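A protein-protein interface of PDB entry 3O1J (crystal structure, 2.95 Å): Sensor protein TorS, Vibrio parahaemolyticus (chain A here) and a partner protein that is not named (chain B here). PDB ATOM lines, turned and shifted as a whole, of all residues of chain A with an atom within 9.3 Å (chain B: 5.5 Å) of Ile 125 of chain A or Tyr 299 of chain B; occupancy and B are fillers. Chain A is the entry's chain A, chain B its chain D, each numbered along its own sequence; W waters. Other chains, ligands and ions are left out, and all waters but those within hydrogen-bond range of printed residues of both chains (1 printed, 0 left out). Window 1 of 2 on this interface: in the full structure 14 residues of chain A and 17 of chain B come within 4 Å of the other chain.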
ATOM      1  N   THR A 117      16.886   6.277   0.125  1.00  0.00           N
ATOM      2  CA  THR A 117      17.827   5.531  -0.692  1.00  0.00           C
ATOM      3  C   THR A 117      17.029   4.826  -1.787  1.00  0.00           C
ATOM      4  O   THR A 117      17.380   4.892  -2.966  1.00  0.00           O
ATOM      5  CB  THR A 117      18.597   4.474   0.146  1.00  0.00           C
ATOM      6  OG1 THR A 117      19.376   5.128   1.156  1.00  0.00           O
ATOM      7  CG2 THR A 117      19.532   3.677  -0.729  1.00  0.00           C
ATOM      8  N   GLN A 118      15.942   4.168  -1.393  1.00  0.00           N
ATOM      9  CA  GLN A 118      15.111   3.456  -2.354  1.00  0.00           C
ATOM     10  C   GLN A 118      14.569   4.398  -3.410  1.00  0.00           C
ATOM     11  O   GLN A 118      14.568   4.070  -4.596  1.00  0.00           O
ATOM     12  CB  GLN A 118      13.953   2.761  -1.654  1.00  0.00           C
ATOM     13  CG  GLN A 118      14.381   1.789  -0.602  1.00  0.00           C
ATOM     14  CD  GLN A 118      13.211   1.032   0.000  1.00  0.00           C
ATOM     15  OE1 GLN A 118      12.496   0.306  -0.709  1.00  0.00           O
ATOM     16  NE2 GLN A 118      13.006   1.195   1.317  1.00  0.00           N
ATOM     17  N   VAL A 119      14.105   5.570  -2.988  1.00  0.00           N
ATOM     18  CA  VAL A 119      13.568   6.525  -3.938  1.00  0.00           C
ATOM     19  C   VAL A 119      14.604   6.842  -5.001  1.00  0.00           C
ATOM     20  O   VAL A 119      14.293   6.883  -6.193  1.00  0.00           O
ATOM     21  CB  VAL A 119      13.127   7.822  -3.252  1.00  0.00           C
ATOM     22  CG1 VAL A 119      12.763   8.875  -4.306  1.00  0.00           C
ATOM     23  CG2 VAL A 119      11.925   7.536  -2.366  1.00  0.00           C
ATOM     24  N   GLN A 120      15.842   7.046  -4.568  1.00  0.00           N
ATOM     25  CA  GLN A 120      16.918   7.354  -5.498  1.00  0.00           C
ATOM     26  C   GLN A 120      17.317   6.183  -6.393  1.00  0.00           C
ATOM     27  O   GLN A 120      17.640   6.376  -7.566  1.00  0.00           O
ATOM     28  CB  GLN A 120      18.125   7.868  -4.730  1.00  0.00           C
ATOM     29  CG  GLN A 120      17.843   9.179  -4.048  1.00  0.00           C
ATOM     30  CD  GLN A 120      19.085   9.811  -3.470  1.00  0.00           C
ATOM     31  OE1 GLN A 120      19.516   9.485  -2.357  1.00  0.00           O
ATOM     32  NE2 GLN A 120      19.682  10.719  -4.233  1.00  0.00           N
ATOM     33  N   ASN A 121      17.309   4.974  -5.840  1.00  0.00           N
ATOM     34  CA  ASN A 121      17.643   3.789  -6.621  1.00  0.00           C
ATOM     35  C   ASN A 121      16.607   3.691  -7.739  1.00  0.00           C
ATOM     36  O   ASN A 121      16.948   3.548  -8.915  1.00  0.00           O
ATOM     37  CB  ASN A 121      17.553   2.509  -5.771  1.00  0.00           C
ATOM     38  CG  ASN A 121      18.661   2.389  -4.734  1.00  0.00           C
ATOM     39  OD1 ASN A 121      19.763   2.906  -4.916  1.00  0.00           O
ATOM     40  ND2 ASN A 121      18.374   1.674  -3.647  1.00  0.00           N
ATOM     41  N   THR A 122      15.336   3.773  -7.359  1.00  0.00           N
ATOM     42  CA  THR A 122      14.252   3.671  -8.322  1.00  0.00           C
ATOM     43  C   THR A 122      14.464   4.651  -9.444  1.00  0.00           C
ATOM     44  O   THR A 122      14.233   4.320 -10.606  1.00  0.00           O
ATOM     45  CB  THR A 122      12.898   3.955  -7.683  1.00  0.00           C
ATOM     46  OG1 THR A 122      12.674   3.025  -6.620  1.00  0.00           O
ATOM     47  CG2 THR A 122      11.778   3.822  -8.715  1.00  0.00           C
ATOM     48  N   SER A 123      14.908   5.854  -9.087  1.00  0.00           N
ATOM     49  CA  SER A 123      15.172   6.904 -10.061  1.00  0.00           C
ATOM     50  C   SER A 123      16.204   6.502 -11.074  1.00  0.00           C
ATOM     51  O   SER A 123      15.939   6.498 -12.272  1.00  0.00           O
ATOM     52  CB  SER A 123      15.678   8.163  -9.381  1.00  0.00           C
ATOM     53  OG  SER A 123      14.594   8.977  -9.009  1.00  0.00           O
ATOM     54  N   THR A 124      17.393   6.171 -10.590  1.00  0.00           N
ATOM     55  CA  THR A 124      18.458   5.803 -11.499  1.00  0.00           C
ATOM     56  C   THR A 124      18.054   4.574 -12.325  1.00  0.00           C
ATOM     57  O   THR A 124      18.282   4.545 -13.547  1.00  0.00           O
ATOM     58  CB  THR A 124      19.789   5.565 -10.746  1.00  0.00           C
ATOM     59  OG1 THR A 124      19.828   4.225 -10.264  1.00  0.00           O
ATOM     60  CG2 THR A 124      19.923   6.530  -9.560  1.00  0.00           C
ATOM     61  N   ILE A 125      17.430   3.581 -11.680  1.00  0.00           N
ATOM     62  CA  ILE A 125      16.987   2.387 -12.390  1.00  0.00           C
ATOM     63  C   ILE A 125      16.086   2.795 -13.560  1.00  0.00           C
ATOM     64  O   ILE A 125      16.234   2.287 -14.668  1.00  0.00           O
ATOM     65  CB  ILE A 125      16.226   1.426 -11.447  1.00  0.00           C
ATOM     66  CG1 ILE A 125      17.195   0.435 -10.804  1.00  0.00           C
ATOM     67  CG2 ILE A 125      15.198   0.629 -12.223  1.00  0.00           C
ATOM     68  CD1 ILE A 125      18.375   1.082 -10.136  1.00  0.00           C
ATOM     69  N   ALA A 126      15.159   3.716 -13.315  1.00  0.00           N
ATOM     70  CA  ALA A 126      14.263   4.183 -14.369  1.00  0.00           C
ATOM     71  C   ALA A 126      15.071   4.709 -15.543  1.00  0.00           C
ATOM     72  O   ALA A 126      14.879   4.255 -16.669  1.00  0.00           O
ATOM     73  CB  ALA A 126      13.348   5.278 -13.853  1.00  0.00           C
ATOM     74  N   VAL A 127      15.965   5.664 -15.287  1.00  0.00           N
ATOM     75  CA  VAL A 127      16.793   6.222 -16.357  1.00  0.00           C
ATOM     76  C   VAL A 127      17.556   5.109 -17.072  1.00  0.00           C
ATOM     77  O   VAL A 127      17.780   5.172 -18.282  1.00  0.00           O
ATOM     78  CB  VAL A 127      17.809   7.259 -15.827  1.00  0.00           C
ATOM     79  CG1 VAL A 127      18.738   7.694 -16.942  1.00  0.00           C
ATOM     80  CG2 VAL A 127      17.082   8.459 -15.290  1.00  0.00           C
ATOM     81  N   ALA A 128      17.956   4.086 -16.328  1.00  0.00           N
ATOM     82  CA  ALA A 128      18.651   2.983 -16.960  1.00  0.00           C
ATOM     83  C   ALA A 128      17.663   2.282 -17.894  1.00  0.00           C
ATOM     84  O   ALA A 128      17.956   2.076 -19.074  1.00  0.00           O
ATOM     85  CB  ALA A 128      19.169   2.008 -15.920  1.00  0.00           C
ATOM     86  N   ASN A 129      16.486   1.931 -17.374  1.00  0.00           N
ATOM     87  CA  ASN A 129      15.475   1.242 -18.178  1.00  0.00           C
ATOM     88  C   ASN A 129      15.116   1.961 -19.473  1.00  0.00           C
ATOM     89  O   ASN A 129      14.792   1.317 -20.476  1.00  0.00           O
ATOM     90  CB  ASN A 129      14.194   1.014 -17.373  1.00  0.00           C
ATOM     91  CG  ASN A 129      14.389   0.048 -16.232  1.00  0.00           C
ATOM     92  OD1 ASN A 129      15.177  -0.886 -16.328  1.00  0.00           O
ATOM     93  ND2 ASN A 129      13.656   0.253 -15.148  1.00  0.00           N
ATOM     94  N   VAL A 130      15.150   3.287 -19.458  1.00  0.00           N
ATOM     95  CA  VAL A 130      14.825   4.022 -20.668  1.00  0.00           C
ATOM     96  C   VAL A 130      16.026   4.018 -21.601  1.00  0.00           C
ATOM     97  O   VAL A 130      15.865   3.986 -22.818  1.00  0.00           O
ATOM     98  CB  VAL A 130      14.396   5.469 -20.362  1.00  0.00           C
ATOM     99  CG1 VAL A 130      14.343   6.273 -21.639  1.00  0.00           C
ATOM    100  CG2 VAL A 130      13.021   5.471 -19.711  1.00  0.00           C
ATOM    101  N   THR A 131      17.230   4.033 -21.038  1.00  0.00           N
ATOM    102  CA  THR A 131      18.434   4.015 -21.866  1.00  0.00           C
ATOM    103  C   THR A 131      18.408   2.744 -22.714  1.00  0.00           C
ATOM    104  O   THR A 131      18.785   2.742 -23.889  1.00  0.00           O
ATOM    105  CB  THR A 131      19.718   4.011 -21.002  1.00  0.00           C
ATOM    106  OG1 THR A 131      19.762   5.191 -20.194  1.00  0.00           O
ATOM    107  CG2 THR A 131      20.950   3.974 -21.881  1.00  0.00           C
ATOM    108  N   HIS A 132      17.942   1.666 -22.099  1.00  0.00           N
ATOM    109  CA  HIS A 132      17.866   0.385 -22.762  1.00  0.00           C
ATOM    110  C   HIS A 132      16.866   0.355 -23.905  1.00  0.00           C
ATOM    111  O   HIS A 132      17.080  -0.346 -24.895  1.00  0.00           O
ATOM    112  CB  HIS A 132      17.506  -0.689 -21.758  1.00  0.00           C
ATOM    113  CG  HIS A 132      17.400  -2.054 -22.356  1.00  0.00           C
ATOM    114  ND1 HIS A 132      16.195  -2.699 -22.533  1.00  0.00           N
ATOM    115  CD2 HIS A 132      18.354  -2.910 -22.794  1.00  0.00           C
ATOM    116  CE1 HIS A 132      16.409  -3.896 -23.048  1.00  0.00           C
ATOM    117  NE2 HIS A 132      17.711  -4.049 -23.215  1.00  0.00           N
ATOM    118  N   ILE A 133      15.770   1.098 -23.771  1.00  0.00           N
ATOM    119  CA  ILE A 133      14.760   1.126 -24.821  1.00  0.00           C
ATOM    120  C   ILE A 133      15.356   1.683 -26.101  1.00  0.00           C
ATOM    121  O   ILE A 133      14.952   1.303 -27.191  1.00  0.00           O
ATOM    122  CB  ILE A 133      13.532   1.967 -24.411  1.00  0.00           C
ATOM    123  CG1 ILE A 133      12.800   1.275 -23.265  1.00  0.00           C
ATOM    124  CG2 ILE A 133      12.585   2.133 -25.590  1.00  0.00           C
ATOM    125  CD1 ILE A 133      11.575   2.008 -22.803  1.00  0.00           C
ATOM    126  N   ALA A 151       6.497  -1.931 -18.918  1.00  0.00           N
ATOM    127  CA  ALA A 151       7.195  -2.103 -17.646  1.00  0.00           C
ATOM    128  C   ALA A 151       7.543  -0.726 -17.087  1.00  0.00           C
ATOM    129  O   ALA A 151       7.641  -0.529 -15.873  1.00  0.00           O
ATOM    130  CB  ALA A 151       8.455  -2.924 -17.860  1.00  0.00           C
ATOM    131  N   LEU A 152       7.722   0.230 -17.990  1.00  0.00           N
ATOM    132  CA  LEU A 152       8.050   1.585 -17.600  1.00  0.00           C
ATOM    133  C   LEU A 152       6.886   2.188 -16.831  1.00  0.00           C
ATOM    134  O   LEU A 152       7.073   2.736 -15.759  1.00  0.00           O
ATOM    135  CB  LEU A 152       8.331   2.426 -18.833  1.00  0.00           C
ATOM    136  CG  LEU A 152       9.257   3.598 -18.559  1.00  0.00           C
ATOM    137  CD1 LEU A 152      10.584   3.034 -18.099  1.00  0.00           C
ATOM    138  CD2 LEU A 152       9.436   4.449 -19.802  1.00  0.00           C
ATOM    139  N   VAL A 155       5.544  -0.509 -13.885  1.00  0.00           N
ATOM    140  CA  VAL A 155       6.506  -0.786 -12.825  1.00  0.00           C
ATOM    141  C   VAL A 155       7.289   0.417 -12.328  1.00  0.00           C
ATOM    142  O   VAL A 155       7.163   0.794 -11.169  1.00  0.00           O
ATOM    143  CB  VAL A 155       7.524  -1.846 -13.255  1.00  0.00           C
ATOM    144  CG1 VAL A 155       8.255  -2.371 -12.045  1.00  0.00           C
ATOM    145  CG2 VAL A 155       6.825  -2.960 -13.979  1.00  0.00           C
ATOM    146  N   ASP A 156       8.105   1.022 -13.183  1.00  0.00           N
ATOM    147  CA  ASP A 156       8.895   2.175 -12.760  1.00  0.00           C
ATOM    148  C   ASP A 156       8.157   3.408 -12.261  1.00  0.00           C
ATOM    149  O   ASP A 156       8.408   3.865 -11.147  1.00  0.00           O
ATOM    150  CB  ASP A 156       9.836   2.577 -13.870  1.00  0.00           C
ATOM    151  CG  ASP A 156      11.053   1.710 -13.904  1.00  0.00           C
ATOM    152  OD1 ASP A 156      11.861   1.818 -12.936  1.00  0.00           O
ATOM    153  OD2 ASP A 156      11.183   0.919 -14.880  1.00  0.00           O
ATOM    154  N   LEU A 157       7.267   3.965 -13.075  1.00  0.00           N
ATOM    155  CA  LEU A 157       6.525   5.148 -12.660  1.00  0.00           C
ATOM    156  C   LEU A 157       5.700   4.837 -11.426  1.00  0.00           C
ATOM    157  O   LEU A 157       5.633   5.636 -10.488  1.00  0.00           O
ATOM    158  CB  LEU A 157       5.608   5.627 -13.781  1.00  0.00           C
ATOM    159  CG  LEU A 157       6.312   6.218 -14.999  1.00  0.00           C
ATOM    160  CD1 LEU A 157       5.285   6.509 -16.077  1.00  0.00           C
ATOM    161  CD2 LEU A 157       7.059   7.476 -14.601  1.00  0.00           C
ATOM    162  N   LEU A 159       6.191   2.545  -9.085  1.00  0.00           N
ATOM    163  CA  LEU A 159       7.041   2.387  -7.917  1.00  0.00           C
ATOM    164  C   LEU A 159       7.557   3.761  -7.474  1.00  0.00           C
ATOM    165  O   LEU A 159       7.713   4.024  -6.285  1.00  0.00           O
ATOM    166  CB  LEU A 159       8.187   1.424  -8.260  1.00  0.00           C
ATOM    167  CG  LEU A 159       8.947   0.661  -7.171  1.00  0.00           C
ATOM    168  CD1 LEU A 159       9.581  -0.583  -7.754  1.00  0.00           C
ATOM    169  CD2 LEU A 159      10.021   1.545  -6.607  1.00  0.00           C
ATOM    170  N   THR A 160       7.801   4.649  -8.427  1.00  0.00           N
ATOM    171  CA  THR A 160       8.262   5.990  -8.092  1.00  0.00           C
ATOM    172  C   THR A 160       7.289   6.716  -7.153  1.00  0.00           C
ATOM    173  O   THR A 160       7.710   7.352  -6.191  1.00  0.00           O
ATOM    174  CB  THR A 160       8.444   6.833  -9.355  1.00  0.00           C
ATOM    175  OG1 THR A 160       9.645   6.427 -10.019  1.00  0.00           O
ATOM    176  CG2 THR A 160       8.514   8.309  -9.012  1.00  0.00           C
ATOM    177  N   ASP A 212      10.849  -6.178  -2.185  1.00  0.00           N
ATOM    178  CA  ASP A 212      12.283  -5.970  -2.117  1.00  0.00           C
ATOM    179  C   ASP A 212      12.720  -6.676  -0.836  1.00  0.00           C
ATOM    180  O   ASP A 212      12.714  -6.087   0.244  1.00  0.00           O
ATOM    181  CB  ASP A 212      12.582  -4.479  -2.025  1.00  0.00           C
ATOM    182  CG  ASP A 212      14.049  -4.175  -2.164  1.00  0.00           C
ATOM    183  OD1 ASP A 212      14.868  -4.945  -1.614  1.00  0.00           O
ATOM    184  OD2 ASP A 212      14.380  -3.160  -2.816  1.00  0.00           O
ATOM    185  N   ARG A 215      15.533  -4.941   1.838  1.00  0.00           N
ATOM    186  CA  ARG A 215      14.927  -3.694   2.298  1.00  0.00           C
ATOM    187  C   ARG A 215      13.632  -3.915   3.082  1.00  0.00           C
ATOM    188  O   ARG A 215      13.486  -3.426   4.207  1.00  0.00           O
ATOM    189  CB  ARG A 215      14.662  -2.780   1.093  1.00  0.00           C
ATOM    190  CG  ARG A 215      15.887  -2.530   0.207  1.00  0.00           C
ATOM    191  CD  ARG A 215      16.954  -1.743   0.940  1.00  0.00           C
ATOM    192  NE  ARG A 215      18.000  -1.204   0.066  1.00  0.00           N
ATOM    193  CZ  ARG A 215      17.786  -0.592  -1.102  1.00  0.00           C
ATOM    194  NH1 ARG A 215      16.559  -0.440  -1.577  1.00  0.00           N
ATOM    195  NH2 ARG A 215      18.804  -0.089  -1.783  1.00  0.00           N
ATOM    196  N   LEU B  21      25.679   1.813  -7.191  1.00  0.00           N
ATOM    197  CA  LEU B  21      24.709   0.814  -7.619  1.00  0.00           C
ATOM    198  C   LEU B  21      25.518  -0.129  -8.501  1.00  0.00           C
ATOM    199  O   LEU B  21      25.370  -1.348  -8.441  1.00  0.00           O
ATOM    200  CB  LEU B  21      23.567   1.477  -8.402  1.00  0.00           C
ATOM    201  CG  LEU B  21      22.314   0.670  -8.765  1.00  0.00           C
ATOM    202  CD1 LEU B  21      22.519  -0.009 -10.083  1.00  0.00           C
ATOM    203  CD2 LEU B  21      22.002  -0.347  -7.691  1.00  0.00           C
ATOM    204  N   ASN B  24      28.199  -2.280  -6.675  1.00  0.00           N
ATOM    205  CA  ASN B  24      27.391  -3.355  -6.125  1.00  0.00           C
ATOM    206  C   ASN B  24      27.188  -4.453  -7.164  1.00  0.00           C
ATOM    207  O   ASN B  24      27.465  -5.628  -6.906  1.00  0.00           O
ATOM    208  CB  ASN B  24      26.036  -2.792  -5.683  1.00  0.00           C
ATOM    209  CG  ASN B  24      25.156  -3.834  -5.023  1.00  0.00           C
ATOM    210  OD1 ASN B  24      24.032  -4.091  -5.473  1.00  0.00           O
ATOM    211  ND2 ASN B  24      25.657  -4.438  -3.949  1.00  0.00           N
ATOM    212  N   TYR B  25      26.696  -4.074  -8.342  1.00  0.00           N
ATOM    213  CA  TYR B  25      26.478  -5.057  -9.399  1.00  0.00           C
ATOM    214  C   TYR B  25      27.751  -5.859  -9.612  1.00  0.00           C
ATOM    215  O   TYR B  25      27.714  -7.075  -9.768  1.00  0.00           O
ATOM    216  CB  TYR B  25      26.113  -4.385 -10.717  1.00  0.00           C
ATOM    217  CG  TYR B  25      26.011  -5.383 -11.848  1.00  0.00           C
ATOM    218  CD1 TYR B  25      24.957  -6.298 -11.905  1.00  0.00           C
ATOM    219  CD2 TYR B  25      26.971  -5.428 -12.853  1.00  0.00           C
ATOM    220  CE1 TYR B  25      24.861  -7.230 -12.939  1.00  0.00           C
ATOM    221  CE2 TYR B  25      26.881  -6.364 -13.894  1.00  0.00           C
ATOM    222  CZ  TYR B  25      25.823  -7.258 -13.929  1.00  0.00           C
ATOM    223  OH  TYR B  25      25.732  -8.167 -14.959  1.00  0.00           O
ATOM    224  N   VAL B  28      28.204  -8.308  -6.431  1.00  0.00           N
ATOM    225  CA  VAL B  28      27.182  -9.347  -6.461  1.00  0.00           C
ATOM    226  C   VAL B  28      27.434 -10.316  -7.619  1.00  0.00           C
ATOM    227  O   VAL B  28      27.413 -11.536  -7.442  1.00  0.00           O
ATOM    228  CB  VAL B  28      25.769  -8.720  -6.589  1.00  0.00           C
ATOM    229  CG1 VAL B  28      24.704  -9.801  -6.549  1.00  0.00           C
ATOM    230  CG2 VAL B  28      25.542  -7.729  -5.459  1.00  0.00           C
ATOM    231  N   SER B 295      25.821  -0.633 -14.108  1.00  0.00           N
ATOM    232  CA  SER B 295      25.010  -1.804 -13.845  1.00  0.00           C
ATOM    233  C   SER B 295      24.036  -1.932 -15.016  1.00  0.00           C
ATOM    234  O   SER B 295      23.665  -0.933 -15.643  1.00  0.00           O
ATOM    235  CB  SER B 295      24.225  -1.631 -12.545  1.00  0.00           C
ATOM    236  OG  SER B 295      23.017  -0.913 -12.765  1.00  0.00           O
ATOM    237  N   PRO B 296      23.613  -3.168 -15.326  1.00  0.00           N
ATOM    238  CA  PRO B 296      22.683  -3.469 -16.411  1.00  0.00           C
ATOM    239  C   PRO B 296      21.334  -2.793 -16.226  1.00  0.00           C
ATOM    240  O   PRO B 296      20.886  -2.537 -15.101  1.00  0.00           O
ATOM    241  CB  PRO B 296      22.574  -4.981 -16.353  1.00  0.00           C
ATOM    242  CG  PRO B 296      23.896  -5.388 -15.849  1.00  0.00           C
ATOM    243  CD  PRO B 296      24.105  -4.416 -14.728  1.00  0.00           C
ATOM    244  N   SER B 297      20.689  -2.537 -17.355  1.00  0.00           N
ATOM    245  CA  SER B 297      19.401  -1.867 -17.410  1.00  0.00           C
ATOM    246  C   SER B 297      18.278  -2.561 -16.671  1.00  0.00           C
ATOM    247  O   SER B 297      17.120  -2.367 -17.019  1.00  0.00           O
ATOM    248  CB  SER B 297      18.967  -1.684 -18.863  1.00  0.00           C
ATOM    249  OG  SER B 297      18.549  -2.926 -19.409  1.00  0.00           O
ATOM    250  N   GLU B 298      18.585  -3.377 -15.677  1.00  0.00           N
ATOM    251  CA  GLU B 298      17.506  -4.022 -14.941  1.00  0.00           C
ATOM    252  C   GLU B 298      17.891  -4.300 -13.500  1.00  0.00           C
ATOM    253  O   GLU B 298      17.036  -4.386 -12.609  1.00  0.00           O
ATOM    254  CB  GLU B 298      17.089  -5.317 -15.641  1.00  0.00           C
ATOM    255  CG  GLU B 298      16.076  -5.131 -16.794  1.00  0.00           C
ATOM    256  CD  GLU B 298      14.756  -4.461 -16.352  1.00  0.00           C
ATOM    257  OE1 GLU B 298      13.766  -4.520 -17.125  1.00  0.00           O
ATOM    258  OE2 GLU B 298      14.710  -3.870 -15.243  1.00  0.00           O
ATOM    259  N   TYR B 299      19.196  -4.404 -13.284  1.00  0.00           N
ATOM    260  CA  TYR B 299      19.748  -4.675 -11.974  1.00  0.00           C
ATOM    261  C   TYR B 299      19.221  -3.751 -10.890  1.00  0.00           C
ATOM    262  O   TYR B 299      19.272  -2.521 -11.001  1.00  0.00           O
ATOM    263  CB  TYR B 299      21.273  -4.584 -12.020  1.00  0.00           C
ATOM    264  CG  TYR B 299      21.923  -4.987 -10.724  1.00  0.00           C
ATOM    265  CD1 TYR B 299      21.844  -6.297 -10.264  1.00  0.00           C
ATOM    266  CD2 TYR B 299      22.572  -4.046  -9.930  1.00  0.00           C
ATOM    267  CE1 TYR B 299      22.390  -6.663  -9.039  1.00  0.00           C
ATOM    268  CE2 TYR B 299      23.120  -4.398  -8.702  1.00  0.00           C
ATOM    269  CZ  TYR B 299      23.023  -5.708  -8.260  1.00  0.00           C
ATOM    270  OH  TYR B 299      23.532  -6.047  -7.027  1.00  0.00           O
ATOM    271  N   ARG B 300      18.724  -4.384  -9.835  1.00  0.00           N
ATOM    272  CA  ARG B 300      18.184  -3.720  -8.659  1.00  0.00           C
ATOM    273  C   ARG B 300      19.193  -4.067  -7.550  1.00  0.00           C
ATOM    274  O   ARG B 300      19.709  -5.180  -7.512  1.00  0.00           O
ATOM    275  CB  ARG B 300      16.820  -4.326  -8.353  1.00  0.00           C
ATOM    276  CG  ARG B 300      15.959  -3.545  -7.390  1.00  0.00           C
ATOM    277  CD  ARG B 300      15.224  -2.431  -8.116  1.00  0.00           C
ATOM    278  NE  ARG B 300      14.594  -2.888  -9.358  1.00  0.00           N
ATOM    279  CZ  ARG B 300      13.817  -2.124 -10.125  1.00  0.00           C
ATOM    280  NH1 ARG B 300      13.566  -0.860  -9.777  1.00  0.00           N
ATOM    281  NH2 ARG B 300      13.294  -2.623 -11.242  1.00  0.00           N
ATOM    282  N   PRO B 301      19.494  -3.126  -6.643  1.00  0.00           N
ATOM    283  CA  PRO B 301      20.451  -3.389  -5.564  1.00  0.00           C
ATOM    284  C   PRO B 301      20.236  -4.746  -4.916  1.00  0.00           C
ATOM    285  O   PRO B 301      19.131  -5.064  -4.489  1.00  0.00           O
ATOM    286  CB  PRO B 301      20.185  -2.254  -4.592  1.00  0.00           C
ATOM    287  CG  PRO B 301      19.820  -1.163  -5.479  1.00  0.00           C
ATOM    288  CD  PRO B 301      18.873  -1.811  -6.455  1.00  0.00           C
ATOM    289  N   THR B 302      21.292  -5.546  -4.848  1.00  0.00           N
ATOM    290  CA  THR B 302      21.210  -6.870  -4.246  1.00  0.00           C
ATOM    291  C   THR B 302      22.159  -6.916  -3.054  1.00  0.00           C
ATOM    292  O   THR B 302      23.309  -6.499  -3.169  1.00  0.00           O
ATOM    293  CB  THR B 302      21.604  -7.953  -5.257  1.00  0.00           C
ATOM    294  OG1 THR B 302      20.678  -7.944  -6.353  1.00  0.00           O
ATOM    295  CG2 THR B 302      21.619  -9.322  -4.587  1.00  0.00           C
HETATM  296  O   HOH W   1      14.714  -2.757 -19.737  1.00  0.00           O
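OD1 of Asn 129 of chain A sits close to OE2 of Glu 298 of chain B.
The side-chain amide oxygen of Asn 129 of chain A lies close to the backbone carbonyl oxygen of Ser 297 of chain B.
The side-chain hydroxyl of Tyr 299 of chain B sits at hydrogen-bond distance from the backbone NH of Thr 302 of chain B, at 3.2 Å.
O of Arg 300 of chain B lies within hydrogen-bond range of OG1 of Thr 302 of chain B (3.1 Å).
The side-chain hydroxyl (OH) of Tyr 299 of chain B is in hydrogen-bond range of the side-chain amide oxygen (OD1) of Asn 24 of chain B (2.5 Å).
The side-chain carboxylate (OD2) of Asp 212 of chain A lies within salt-bridge range of the guanidinium group (NH1) of Arg 215 of chain A (3.7 Å).
The side-chain amide nitrogen (ND2) of Asn 121 of chain A sits close to the guanidinium group (NH2) of Arg 215 of chain A, at 2.6 Å.
The side-chain amide nitrogen (ND2) of Asn 129 of chain A sits close to the backbone carbonyl oxygen (O) of Ile 125 of chain A.
Among the printed residues, pairs that only touch across the chains: Asn 121 of chain A with Pro 301 of chain B (3.7 Å), Ile 125 of chain A with Tyr 299 of chain B (3.6 Å), Ile 125 of chain A with Arg 300 of chain B (3.3 Å), Ala 128 of chain A with Ser 297 of chain B (3.9 Å), His 132 of chain A with Ser 297 of chain B (3.3 Å) and Arg 215 of chain A with Pro 301 of chain B (3.8 Å).
Ile 125 of chain A touches just these residues of chain B: Tyr 299 (3.6 Å) and Arg 300 (3.3 Å).
Val 155 of chain A touches none of the printed residues of chain B.
Printed residues of chain B within 4 Å of Arg 215 of chain A: Pro 301 (3.8 Å).
Leu 21 of chain B touches none of the printed residues of chain A.
No residue of chain A comes within 4 Å of Pro 296 of chain B.
Printed residues of chain A within 4 Å of Glu 298 of chain B: Asn 129 (3.2 Å).
Of the printed residues of chain A, Tyr 299 of chain B touches Ile 125.
No residue of chain A comes within 4 Å of Thr 302 of chain B.
The nearest residue of chain B that does not touch Ile 125 of chain A is Leu 21 of chain B (4.2 Å).
The nearest residue of chain A that does not touch Tyr 299 of chain B is Asn 129 of chain A (6.1 Å).
The nearest printed residue of chain B that does not touch His 132 of chain A is Glu 298 of chain B (6.2 Å).
Hydrophobic or aromatic side chains of chain A that line the printed part of chain B: Ile 125 and His 132.
Of the 12 printed residues of chain B, 5 touch a printed residue of chain A.
Hydrophobic or aromatic side chains of chain B that line the printed part of chain A: Pro 301.
Along chain B the printed residues that touch a printed residue of chain A span positions 297 to 301.
Among the printed residues, 8 pairs touch across the chains.
Among the printed residues, no Asp or Glu carboxylate lies within 4 Å of a Lys or Arg side-chain nitrogen of the other chain.
Water W1 bridges ND1 of His 132 of chain A and OE1 of Glu 298 of chain B.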
